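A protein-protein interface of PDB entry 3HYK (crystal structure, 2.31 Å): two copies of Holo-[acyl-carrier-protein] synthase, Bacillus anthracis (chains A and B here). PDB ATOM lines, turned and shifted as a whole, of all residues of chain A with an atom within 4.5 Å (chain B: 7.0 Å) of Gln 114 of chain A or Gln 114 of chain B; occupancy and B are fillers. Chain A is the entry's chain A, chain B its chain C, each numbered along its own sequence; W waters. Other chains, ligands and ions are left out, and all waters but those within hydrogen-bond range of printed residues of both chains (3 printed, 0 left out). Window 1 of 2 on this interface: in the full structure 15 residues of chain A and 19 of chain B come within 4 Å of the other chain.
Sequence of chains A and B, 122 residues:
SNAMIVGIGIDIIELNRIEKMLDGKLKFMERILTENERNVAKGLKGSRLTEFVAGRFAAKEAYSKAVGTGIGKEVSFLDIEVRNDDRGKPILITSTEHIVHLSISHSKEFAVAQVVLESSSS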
ATOM      1  N   ILE A   8     -17.126   3.204  -8.836  1.00  0.00           N
ATOM      2  CA  ILE A   8     -17.016   4.503  -9.506  1.00  0.00           C
ATOM      3  C   ILE A   8     -17.604   5.580  -8.594  1.00  0.00           C
ATOM      4  O   ILE A   8     -18.450   5.292  -7.749  1.00  0.00           O
ATOM      5  CB  ILE A   8     -17.723   4.508 -10.924  1.00  0.00           C
ATOM      6  CG1 ILE A   8     -19.246   4.664 -10.818  1.00  0.00           C
ATOM      7  CG2 ILE A   8     -17.378   3.232 -11.693  1.00  0.00           C
ATOM      8  CD1 ILE A   8     -19.972   4.665 -12.210  1.00  0.00           C
ATOM      9  N   GLY A   9     -17.150   6.816  -8.768  1.00  0.00           N
ATOM     10  CA  GLY A   9     -17.626   7.930  -7.983  1.00  0.00           C
ATOM     11  C   GLY A   9     -17.627   9.228  -8.759  1.00  0.00           C
ATOM     12  O   GLY A   9     -16.751   9.460  -9.595  1.00  0.00           O
ATOM     13  N   ILE A  10     -18.629  10.064  -8.512  1.00  0.00           N
ATOM     14  CA  ILE A  10     -18.716  11.361  -9.182  1.00  0.00           C
ATOM     15  C   ILE A  10     -19.122  12.394  -8.136  1.00  0.00           C
ATOM     16  O   ILE A  10     -19.753  12.059  -7.141  1.00  0.00           O
ATOM     17  CB  ILE A  10     -19.749  11.371 -10.354  1.00  0.00           C
ATOM     18  CG1 ILE A  10     -19.483  12.534 -11.324  1.00  0.00           C
ATOM     19  CG2 ILE A  10     -21.160  11.421  -9.818  1.00  0.00           C
ATOM     20  CD1 ILE A  10     -20.404  12.575 -12.563  1.00  0.00           C
ATOM     21  N   ALA A  62     -15.187  12.147  -4.650  1.00  0.00           N
ATOM     22  CA  ALA A  62     -15.579  11.216  -5.682  1.00  0.00           C
ATOM     23  C   ALA A  62     -14.858   9.869  -5.452  1.00  0.00           C
ATOM     24  O   ALA A  62     -15.449   8.804  -5.642  1.00  0.00           O
ATOM     25  CB  ALA A  62     -15.258  11.777  -7.061  1.00  0.00           C
ATOM     26  N   HIS A 101      -8.347   5.912 -11.437  1.00  0.00           N
ATOM     27  CA  HIS A 101      -8.463   6.778 -12.604  1.00  0.00           C
ATOM     28  C   HIS A 101      -9.281   7.990 -12.159  1.00  0.00           C
ATOM     29  O   HIS A 101     -10.323   7.853 -11.513  1.00  0.00           O
ATOM     30  CB  HIS A 101      -9.109   6.064 -13.792  1.00  0.00           C
ATOM     31  CG  HIS A 101      -8.397   4.802 -14.186  1.00  0.00           C
ATOM     32  ND1 HIS A 101      -7.255   4.795 -14.961  1.00  0.00           N
ATOM     33  CD2 HIS A 101      -8.659   3.508 -13.892  1.00  0.00           C
ATOM     34  CE1 HIS A 101      -6.846   3.550 -15.119  1.00  0.00           C
ATOM     35  NE2 HIS A 101      -7.682   2.750 -14.484  1.00  0.00           N
ATOM     36  N   LEU A 102      -8.793   9.173 -12.503  1.00  0.00           N
ATOM     37  CA  LEU A 102      -9.427  10.427 -12.122  1.00  0.00           C
ATOM     38  C   LEU A 102      -9.457  11.448 -13.239  1.00  0.00           C
ATOM     39  O   LEU A 102      -8.608  11.454 -14.124  1.00  0.00           O
ATOM     40  CB  LEU A 102      -8.616  11.017 -10.969  1.00  0.00           C
ATOM     41  CG  LEU A 102      -8.807  12.448 -10.510  1.00  0.00           C
ATOM     42  CD1 LEU A 102     -10.167  12.643  -9.881  1.00  0.00           C
ATOM     43  CD2 LEU A 102      -7.689  12.770  -9.536  1.00  0.00           C
ATOM     44  N   SER A 103     -10.460  12.311 -13.182  1.00  0.00           N
ATOM     45  CA  SER A 103     -10.583  13.441 -14.089  1.00  0.00           C
ATOM     46  C   SER A 103     -11.316  14.539 -13.326  1.00  0.00           C
ATOM     47  O   SER A 103     -12.166  14.253 -12.468  1.00  0.00           O
ATOM     48  CB  SER A 103     -11.335  13.087 -15.359  1.00  0.00           C
ATOM     49  OG  SER A 103     -11.287  14.179 -16.273  1.00  0.00           O
ATOM     50  N   ALA A 113     -15.753  16.094 -10.604  1.00  0.00           N
ATOM     51  CA  ALA A 113     -14.677  15.111 -10.555  1.00  0.00           C
ATOM     52  C   ALA A 113     -15.301  13.748 -10.685  1.00  0.00           C
ATOM     53  O   ALA A 113     -16.460  13.549 -10.320  1.00  0.00           O
ATOM     54  CB  ALA A 113     -13.877  15.216  -9.261  1.00  0.00           C
ATOM     55  N   GLN A 114     -14.554  12.827 -11.281  1.00  0.00           N
ATOM     56  CA  GLN A 114     -14.997  11.458 -11.395  1.00  0.00           C
ATOM     57  C   GLN A 114     -13.825  10.526 -11.176  1.00  0.00           C
ATOM     58  O   GLN A 114     -12.678  10.816 -11.526  1.00  0.00           O
ATOM     59  CB  GLN A 114     -15.646  11.147 -12.747  1.00  0.00           C
ATOM     60  CG  GLN A 114     -14.722  11.261 -13.956  1.00  0.00           C
ATOM     61  CD  GLN A 114     -15.287  10.561 -15.193  1.00  0.00           C
ATOM     62  OE1 GLN A 114     -14.876  10.832 -16.317  1.00  0.00           O
ATOM     63  NE2 GLN A 114     -16.213   9.647 -14.978  1.00  0.00           N
ATOM     64  N   VAL A 115     -14.128   9.385 -10.598  1.00  0.00           N
ATOM     65  CA  VAL A 115     -13.127   8.389 -10.344  1.00  0.00           C
ATOM     66  C   VAL A 115     -13.664   7.034 -10.732  1.00  0.00           C
ATOM     67  O   VAL A 115     -14.866   6.746 -10.567  1.00  0.00           O
ATOM     68  CB  VAL A 115     -12.730   8.345  -8.839  1.00  0.00           C
ATOM     69  CG1 VAL A 115     -12.019   7.025  -8.503  1.00  0.00           C
ATOM     70  CG2 VAL A 115     -11.907   9.573  -8.476  1.00  0.00           C
ATOM     71  N   VAL A 116     -12.754   6.225 -11.270  1.00  0.00           N
ATOM     72  CA  VAL A 116     -13.026   4.834 -11.588  1.00  0.00           C
ATOM     73  C   VAL A 116     -11.884   4.082 -10.955  1.00  0.00           C
ATOM     74  O   VAL A 116     -10.721   4.371 -11.226  1.00  0.00           O
ATOM     75  CB  VAL A 116     -13.087   4.552 -13.105  1.00  0.00           C
ATOM     76  CG1 VAL A 116     -13.162   3.044 -13.380  1.00  0.00           C
ATOM     77  CG2 VAL A 116     -14.281   5.279 -13.725  1.00  0.00           C
ATOM     78  N   ILE B   8     -21.197   3.405 -21.148  1.00  0.00           N
ATOM     79  CA  ILE B   8     -21.168   4.367 -20.054  1.00  0.00           C
ATOM     80  C   ILE B   8     -22.327   5.359 -20.264  1.00  0.00           C
ATOM     81  O   ILE B   8     -22.839   5.503 -21.367  1.00  0.00           O
ATOM     82  CB  ILE B   8     -19.751   5.078 -19.906  1.00  0.00           C
ATOM     83  CG1 ILE B   8     -19.517   6.176 -20.936  1.00  0.00           C
ATOM     84  CG2 ILE B   8     -18.598   4.042 -19.996  1.00  0.00           C
ATOM     85  CD1 ILE B   8     -18.146   6.850 -20.783  1.00  0.00           C
ATOM     86  N   GLY B   9     -22.760   6.020 -19.202  1.00  0.00           N
ATOM     87  CA  GLY B   9     -23.862   6.973 -19.301  1.00  0.00           C
ATOM     88  C   GLY B   9     -23.696   8.050 -18.259  1.00  0.00           C
ATOM     89  O   GLY B   9     -23.268   7.771 -17.129  1.00  0.00           O
ATOM     90  N   ILE B  10     -23.985   9.285 -18.650  1.00  0.00           N
ATOM     91  CA  ILE B  10     -23.893  10.441 -17.746  1.00  0.00           C
ATOM     92  C   ILE B  10     -25.166  11.236 -17.880  1.00  0.00           C
ATOM     93  O   ILE B  10     -25.740  11.298 -18.974  1.00  0.00           O
ATOM     94  CB  ILE B  10     -22.718  11.416 -18.094  1.00  0.00           C
ATOM     95  CG1 ILE B  10     -22.532  12.484 -17.031  1.00  0.00           C
ATOM     96  CG2 ILE B  10     -22.927  12.146 -19.412  1.00  0.00           C
ATOM     97  CD1 ILE B  10     -21.697  12.059 -15.922  1.00  0.00           C
ATOM     98  N   ASP B  11     -25.616  11.841 -16.786  1.00  0.00           N
ATOM     99  CA  ASP B  11     -26.786  12.686 -16.862  1.00  0.00           C
ATOM    100  C   ASP B  11     -26.704  13.860 -15.902  1.00  0.00           C
ATOM    101  O   ASP B  11     -26.297  13.672 -14.762  1.00  0.00           O
ATOM    102  CB  ASP B  11     -28.055  11.897 -16.547  1.00  0.00           C
ATOM    103  CG  ASP B  11     -29.318  12.655 -16.962  1.00  0.00           C
ATOM    104  OD1 ASP B  11     -29.269  13.374 -17.980  1.00  0.00           O
ATOM    105  OD2 ASP B  11     -30.356  12.500 -16.306  1.00  0.00           O
ATOM    106  N   ALA B  58     -31.941  10.877 -12.934  1.00  0.00           N
ATOM    107  CA  ALA B  58     -30.645  10.920 -13.588  1.00  0.00           C
ATOM    108  C   ALA B  58     -29.913   9.556 -13.592  1.00  0.00           C
ATOM    109  O   ALA B  58     -29.307   9.165 -14.591  1.00  0.00           O
ATOM    110  CB  ALA B  58     -29.788  12.017 -12.955  1.00  0.00           C
ATOM    111  N   ALA B  59     -29.999   8.812 -12.499  1.00  0.00           N
ATOM    112  CA  ALA B  59     -29.352   7.512 -12.429  1.00  0.00           C
ATOM    113  C   ALA B  59     -29.946   6.586 -13.483  1.00  0.00           C
ATOM    114  O   ALA B  59     -29.222   5.871 -14.214  1.00  0.00           O
ATOM    115  CB  ALA B  59     -29.552   6.917 -11.059  1.00  0.00           C
ATOM    116  N   ALA B  62     -29.143   7.824 -17.043  1.00  0.00           N
ATOM    117  CA  ALA B  62     -27.755   7.549 -17.344  1.00  0.00           C
ATOM    118  C   ALA B  62     -27.558   6.040 -17.613  1.00  0.00           C
ATOM    119  O   ALA B  62     -26.765   5.642 -18.475  1.00  0.00           O
ATOM    120  CB  ALA B  62     -26.862   8.046 -16.198  1.00  0.00           C
ATOM    121  N   TYR B  63     -28.256   5.199 -16.860  1.00  0.00           N
ATOM    122  CA  TYR B  63     -28.197   3.761 -17.101  1.00  0.00           C
ATOM    123  C   TYR B  63     -28.673   3.452 -18.530  1.00  0.00           C
ATOM    124  O   TYR B  63     -28.008   2.734 -19.289  1.00  0.00           O
ATOM    125  CB  TYR B  63     -29.059   3.002 -16.077  1.00  0.00           C
ATOM    126  CG  TYR B  63     -29.252   1.562 -16.457  1.00  0.00           C
ATOM    127  CD1 TYR B  63     -28.243   0.634 -16.254  1.00  0.00           C
ATOM    128  CD2 TYR B  63     -30.438   1.130 -17.045  1.00  0.00           C
ATOM    129  CE1 TYR B  63     -28.404  -0.671 -16.624  1.00  0.00           C
ATOM    130  CE2 TYR B  63     -30.596  -0.185 -17.451  1.00  0.00           C
ATOM    131  CZ  TYR B  63     -29.573  -1.079 -17.225  1.00  0.00           C
ATOM    132  OH  TYR B  63     -29.718  -2.396 -17.563  1.00  0.00           O
ATOM    133  N   HIS B 101     -22.405  -0.238 -12.467  1.00  0.00           N
ATOM    134  CA  HIS B 101     -21.700   0.668 -11.568  1.00  0.00           C
ATOM    135  C   HIS B 101     -22.399   2.004 -11.687  1.00  0.00           C
ATOM    136  O   HIS B 101     -22.685   2.467 -12.785  1.00  0.00           O
ATOM    137  CB  HIS B 101     -20.229   0.779 -11.914  1.00  0.00           C
ATOM    138  CG  HIS B 101     -19.524  -0.536 -11.904  1.00  0.00           C
ATOM    139  ND1 HIS B 101     -19.173  -1.182 -10.736  1.00  0.00           N
ATOM    140  CD2 HIS B 101     -19.106  -1.329 -12.918  1.00  0.00           C
ATOM    141  CE1 HIS B 101     -18.577  -2.322 -11.036  1.00  0.00           C
ATOM    142  NE2 HIS B 101     -18.526  -2.437 -12.351  1.00  0.00           N
ATOM    143  N   LEU B 102     -22.678   2.610 -10.539  1.00  0.00           N
ATOM    144  CA  LEU B 102     -23.402   3.877 -10.458  1.00  0.00           C
ATOM    145  C   LEU B 102     -22.876   4.840  -9.406  1.00  0.00           C
ATOM    146  O   LEU B 102     -22.359   4.419  -8.374  1.00  0.00           O
ATOM    147  CB  LEU B 102     -24.851   3.565 -10.070  1.00  0.00           C
ATOM    148  CG  LEU B 102     -25.756   4.718  -9.653  1.00  0.00           C
ATOM    149  CD1 LEU B 102     -26.065   5.651 -10.823  1.00  0.00           C
ATOM    150  CD2 LEU B 102     -27.028   4.123  -9.064  1.00  0.00           C
ATOM    151  N   SER B 103     -23.006   6.138  -9.684  1.00  0.00           N
ATOM    152  CA  SER B 103     -22.686   7.170  -8.689  1.00  0.00           C
ATOM    153  C   SER B 103     -23.622   8.378  -8.900  1.00  0.00           C
ATOM    154  O   SER B 103     -24.029   8.689 -10.027  1.00  0.00           O
ATOM    155  CB  SER B 103     -21.216   7.598  -8.716  1.00  0.00           C
ATOM    156  OG  SER B 103     -20.929   8.511  -7.643  1.00  0.00           O
ATOM    157  N   ILE B 104     -23.955   9.037  -7.802  1.00  0.00           N
ATOM    158  CA  ILE B 104     -24.820  10.198  -7.807  1.00  0.00           C
ATOM    159  C   ILE B 104     -24.186  11.324  -6.973  1.00  0.00           C
ATOM    160  O   ILE B 104     -23.449  11.064  -6.011  1.00  0.00           O
ATOM    161  CB  ILE B 104     -26.197   9.839  -7.171  1.00  0.00           C
ATOM    162  CG1 ILE B 104     -26.906   8.734  -7.962  1.00  0.00           C
ATOM    163  CG2 ILE B 104     -27.117  11.055  -7.075  1.00  0.00           C
ATOM    164  CD1 ILE B 104     -28.226   8.274  -7.324  1.00  0.00           C
ATOM    165  N   SER B 105     -24.468  12.564  -7.355  1.00  0.00           N
ATOM    166  CA  SER B 105     -24.057  13.734  -6.590  1.00  0.00           C
ATOM    167  C   SER B 105     -25.101  14.802  -6.826  1.00  0.00           C
ATOM    168  O   SER B 105     -25.695  14.868  -7.905  1.00  0.00           O
ATOM    169  CB  SER B 105     -22.684  14.286  -6.985  1.00  0.00           C
ATOM    170  OG  SER B 105     -22.338  15.415  -6.173  1.00  0.00           O
ATOM    171  N   VAL B 112     -26.294  14.969 -10.658  1.00  0.00           N
ATOM    172  CA  VAL B 112     -25.582  14.273 -11.707  1.00  0.00           C
ATOM    173  C   VAL B 112     -25.511  12.822 -11.312  1.00  0.00           C
ATOM    174  O   VAL B 112     -25.525  12.477 -10.127  1.00  0.00           O
ATOM    175  CB  VAL B 112     -24.166  14.835 -11.961  1.00  0.00           C
ATOM    176  CG1 VAL B 112     -24.271  16.243 -12.470  1.00  0.00           C
ATOM    177  CG2 VAL B 112     -23.309  14.789 -10.686  1.00  0.00           C
ATOM    178  N   ALA B 113     -25.487  11.963 -12.321  1.00  0.00           N
ATOM    179  CA  ALA B 113     -25.374  10.537 -12.102  1.00  0.00           C
ATOM    180  C   ALA B 113     -24.606   9.995 -13.270  1.00  0.00           C
ATOM    181  O   ALA B 113     -24.695  10.541 -14.374  1.00  0.00           O
ATOM    182  CB  ALA B 113     -26.755   9.874 -12.016  1.00  0.00           C
ATOM    183  N   GLN B 114     -23.826   8.945 -13.026  1.00  0.00           N
ATOM    184  CA  GLN B 114     -23.089   8.290 -14.081  1.00  0.00           C
ATOM    185  C   GLN B 114     -23.183   6.779 -13.889  1.00  0.00           C
ATOM    186  O   GLN B 114     -23.302   6.275 -12.767  1.00  0.00           O
ATOM    187  CB  GLN B 114     -21.610   8.705 -14.099  1.00  0.00           C
ATOM    188  CG  GLN B 114     -20.848   8.382 -12.813  1.00  0.00           C
ATOM    189  CD  GLN B 114     -19.328   8.497 -12.968  1.00  0.00           C
ATOM    190  OE1 GLN B 114     -18.804   8.423 -14.075  1.00  0.00           O
ATOM    191  NE2 GLN B 114     -18.622   8.628 -11.856  1.00  0.00           N
ATOM    192  N   VAL B 115     -23.108   6.072 -15.006  1.00  0.00           N
ATOM    193  CA  VAL B 115     -23.150   4.629 -15.005  1.00  0.00           C
ATOM    194  C   VAL B 115     -22.081   4.070 -15.940  1.00  0.00           C
ATOM    195  O   VAL B 115     -21.775   4.647 -17.000  1.00  0.00           O
ATOM    196  CB  VAL B 115     -24.556   4.091 -15.416  1.00  0.00           C
ATOM    197  CG1 VAL B 115     -24.502   2.592 -15.753  1.00  0.00           C
ATOM    198  CG2 VAL B 115     -25.600   4.389 -14.321  1.00  0.00           C
ATOM    199  N   VAL B 116     -21.478   2.977 -15.482  1.00  0.00           N
ATOM    200  CA  VAL B 116     -20.519   2.196 -16.260  1.00  0.00           C
ATOM    201  C   VAL B 116     -21.085   0.797 -16.182  1.00  0.00           C
ATOM    202  O   VAL B 116     -21.377   0.301 -15.083  1.00  0.00           O
ATOM    203  CB  VAL B 116     -19.100   2.215 -15.699  1.00  0.00           C
ATOM    204  CG1 VAL B 116     -18.172   1.297 -16.518  1.00  0.00           C
ATOM    205  CG2 VAL B 116     -18.568   3.657 -15.690  1.00  0.00           C
HETATM  206  O   HOH W   1     -20.856   5.001  -6.073  1.00  0.00           O
HETATM  207  O   HOH W   2     -16.271   7.734 -12.831  1.00  0.00           O
HETATM  208  O   HOH W   3     -19.879   2.235  -7.841  1.00  0.00           O
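The backbone carbonyl oxygen (O) of Gly 9 of chain A sits at hydrogen-bond distance from the side-chain amide nitrogen (NE2) of Gln 114 of chain B (3.1 Å). The side-chain hydroxyl (OG) of Ser 103 of chain B lies within hydrogen-bond range of the backbone NH (N) of Ile 10 of chain A. The side-chain amide nitrogen of Gln 114 of chain A sits at hydrogen-bond distance from the side-chain amide oxygen of Gln 114 of chain B (3.0 Å).
O of Gly 9 of chain A sits at hydrogen-bond distance from N of Val 115 of chain A (2.8 Å). N of Gln 114 of chain A lies within hydrogen-bond range of O of Ser 103 of chain A (3.0 Å). N of His 101 of chain B is in hydrogen-bond range of O of Val 116 of chain B (2.9 Å). The backbone carbonyl oxygen (O) of Ser 103 of chain B lies within hydrogen-bond range of the backbone NH (N) of Gln 114 of chain B, at 3.0 Å. N of Val 112 of chain B is in hydrogen-bond range of O of Ser 105 of chain B (2.8 Å).
Among the printed residues, merely in contact across the chains: Ile 8 of chain A with His 101 of chain B, Ile 8 of chain A with Leu 102 of chain B, Ile 8 of chain A with Ser 103 of chain B, Ile 8 of chain A with Gln 114 of chain B, Ile 8 of chain A with Val 116 of chain B, Gly 9 of chain A with Ser 103 of chain B, Ile 10 of chain A with Ile 10 of chain B, Ile 10 of chain A with Ile 104 of chain B, Ile 10 of chain A with Ser 105 of chain B and Ile 10 of chain A with Gln 114 of chain B.
Of the printed residues of chain B, Gly 9 of chain A touches Ser 103 (3.4 Å) and Gln 114 (3.1 Å). Ser 103 of chain A touches none of the printed residues of chain B. Gln 114 of chain A touches one residue of chain B. Ala 59 of chain B touches none of the printed residues of chain A. Printed residues of chain A within 4 Å of Ile 104 of chain B: Ile 10 (3.99 Å). Gln 114 of chain B touches just these residues of chain A: Ile 8 (3.7 Å), Gly 9 (3.1 Å), Ile 10 (3.3 Å) and Gln 114 (3.0 Å). The nearest residue of chain A that does not touch Gln 114 of chain B is Val 115 of chain A (4.4 Å).
Printed residues of chain A that touch a printed residue of chain B: Ile 8, Gly 9, Ile 10 and Gln 114. Along chain A the printed residues that touch a printed residue of chain B span positions 8 to 114.
Ile 8 of chain A touches Leu 102 of chain B, but with the chains exchanged Leu 102 of chain A does not touch Ile 8 of chain B (12.4 Å). Ile 10 of chain B touches its own counterpart, Ile 10 of chain A. Ile 10 of chain A touches Ser 103 of chain B, but with the chains exchanged Ser 103 of chain A does not touch Ile 10 of chain B (10.4 Å). Gln 114 of chain A touches its own counterpart, Gln 114 of chain B. 11 positions are printed for both chains. Of the 13 pairs that touch across the chains among the printed residues, 2 have their exchanged pair printed and touching as well.
Water W2 lies within hydrogen-bond range of NE2 of Gln 114 of chain B (2.7 Å), O of Val 115 of chain A (2.8 Å) and NE2 of Gln 114 of chain A (2.9 Å). Water W1 bridges the backbone carbonyl oxygen (O) of Leu 102 of chain B (2.8 Å) and the backbone carbonyl oxygen (O) of Ile 8 of chain A (2.9 Å). Water W3 lies within hydrogen-bond range of the backbone NH of Ile 8 of chain A and the backbone carbonyl oxygen of Leu 102 of chain B.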
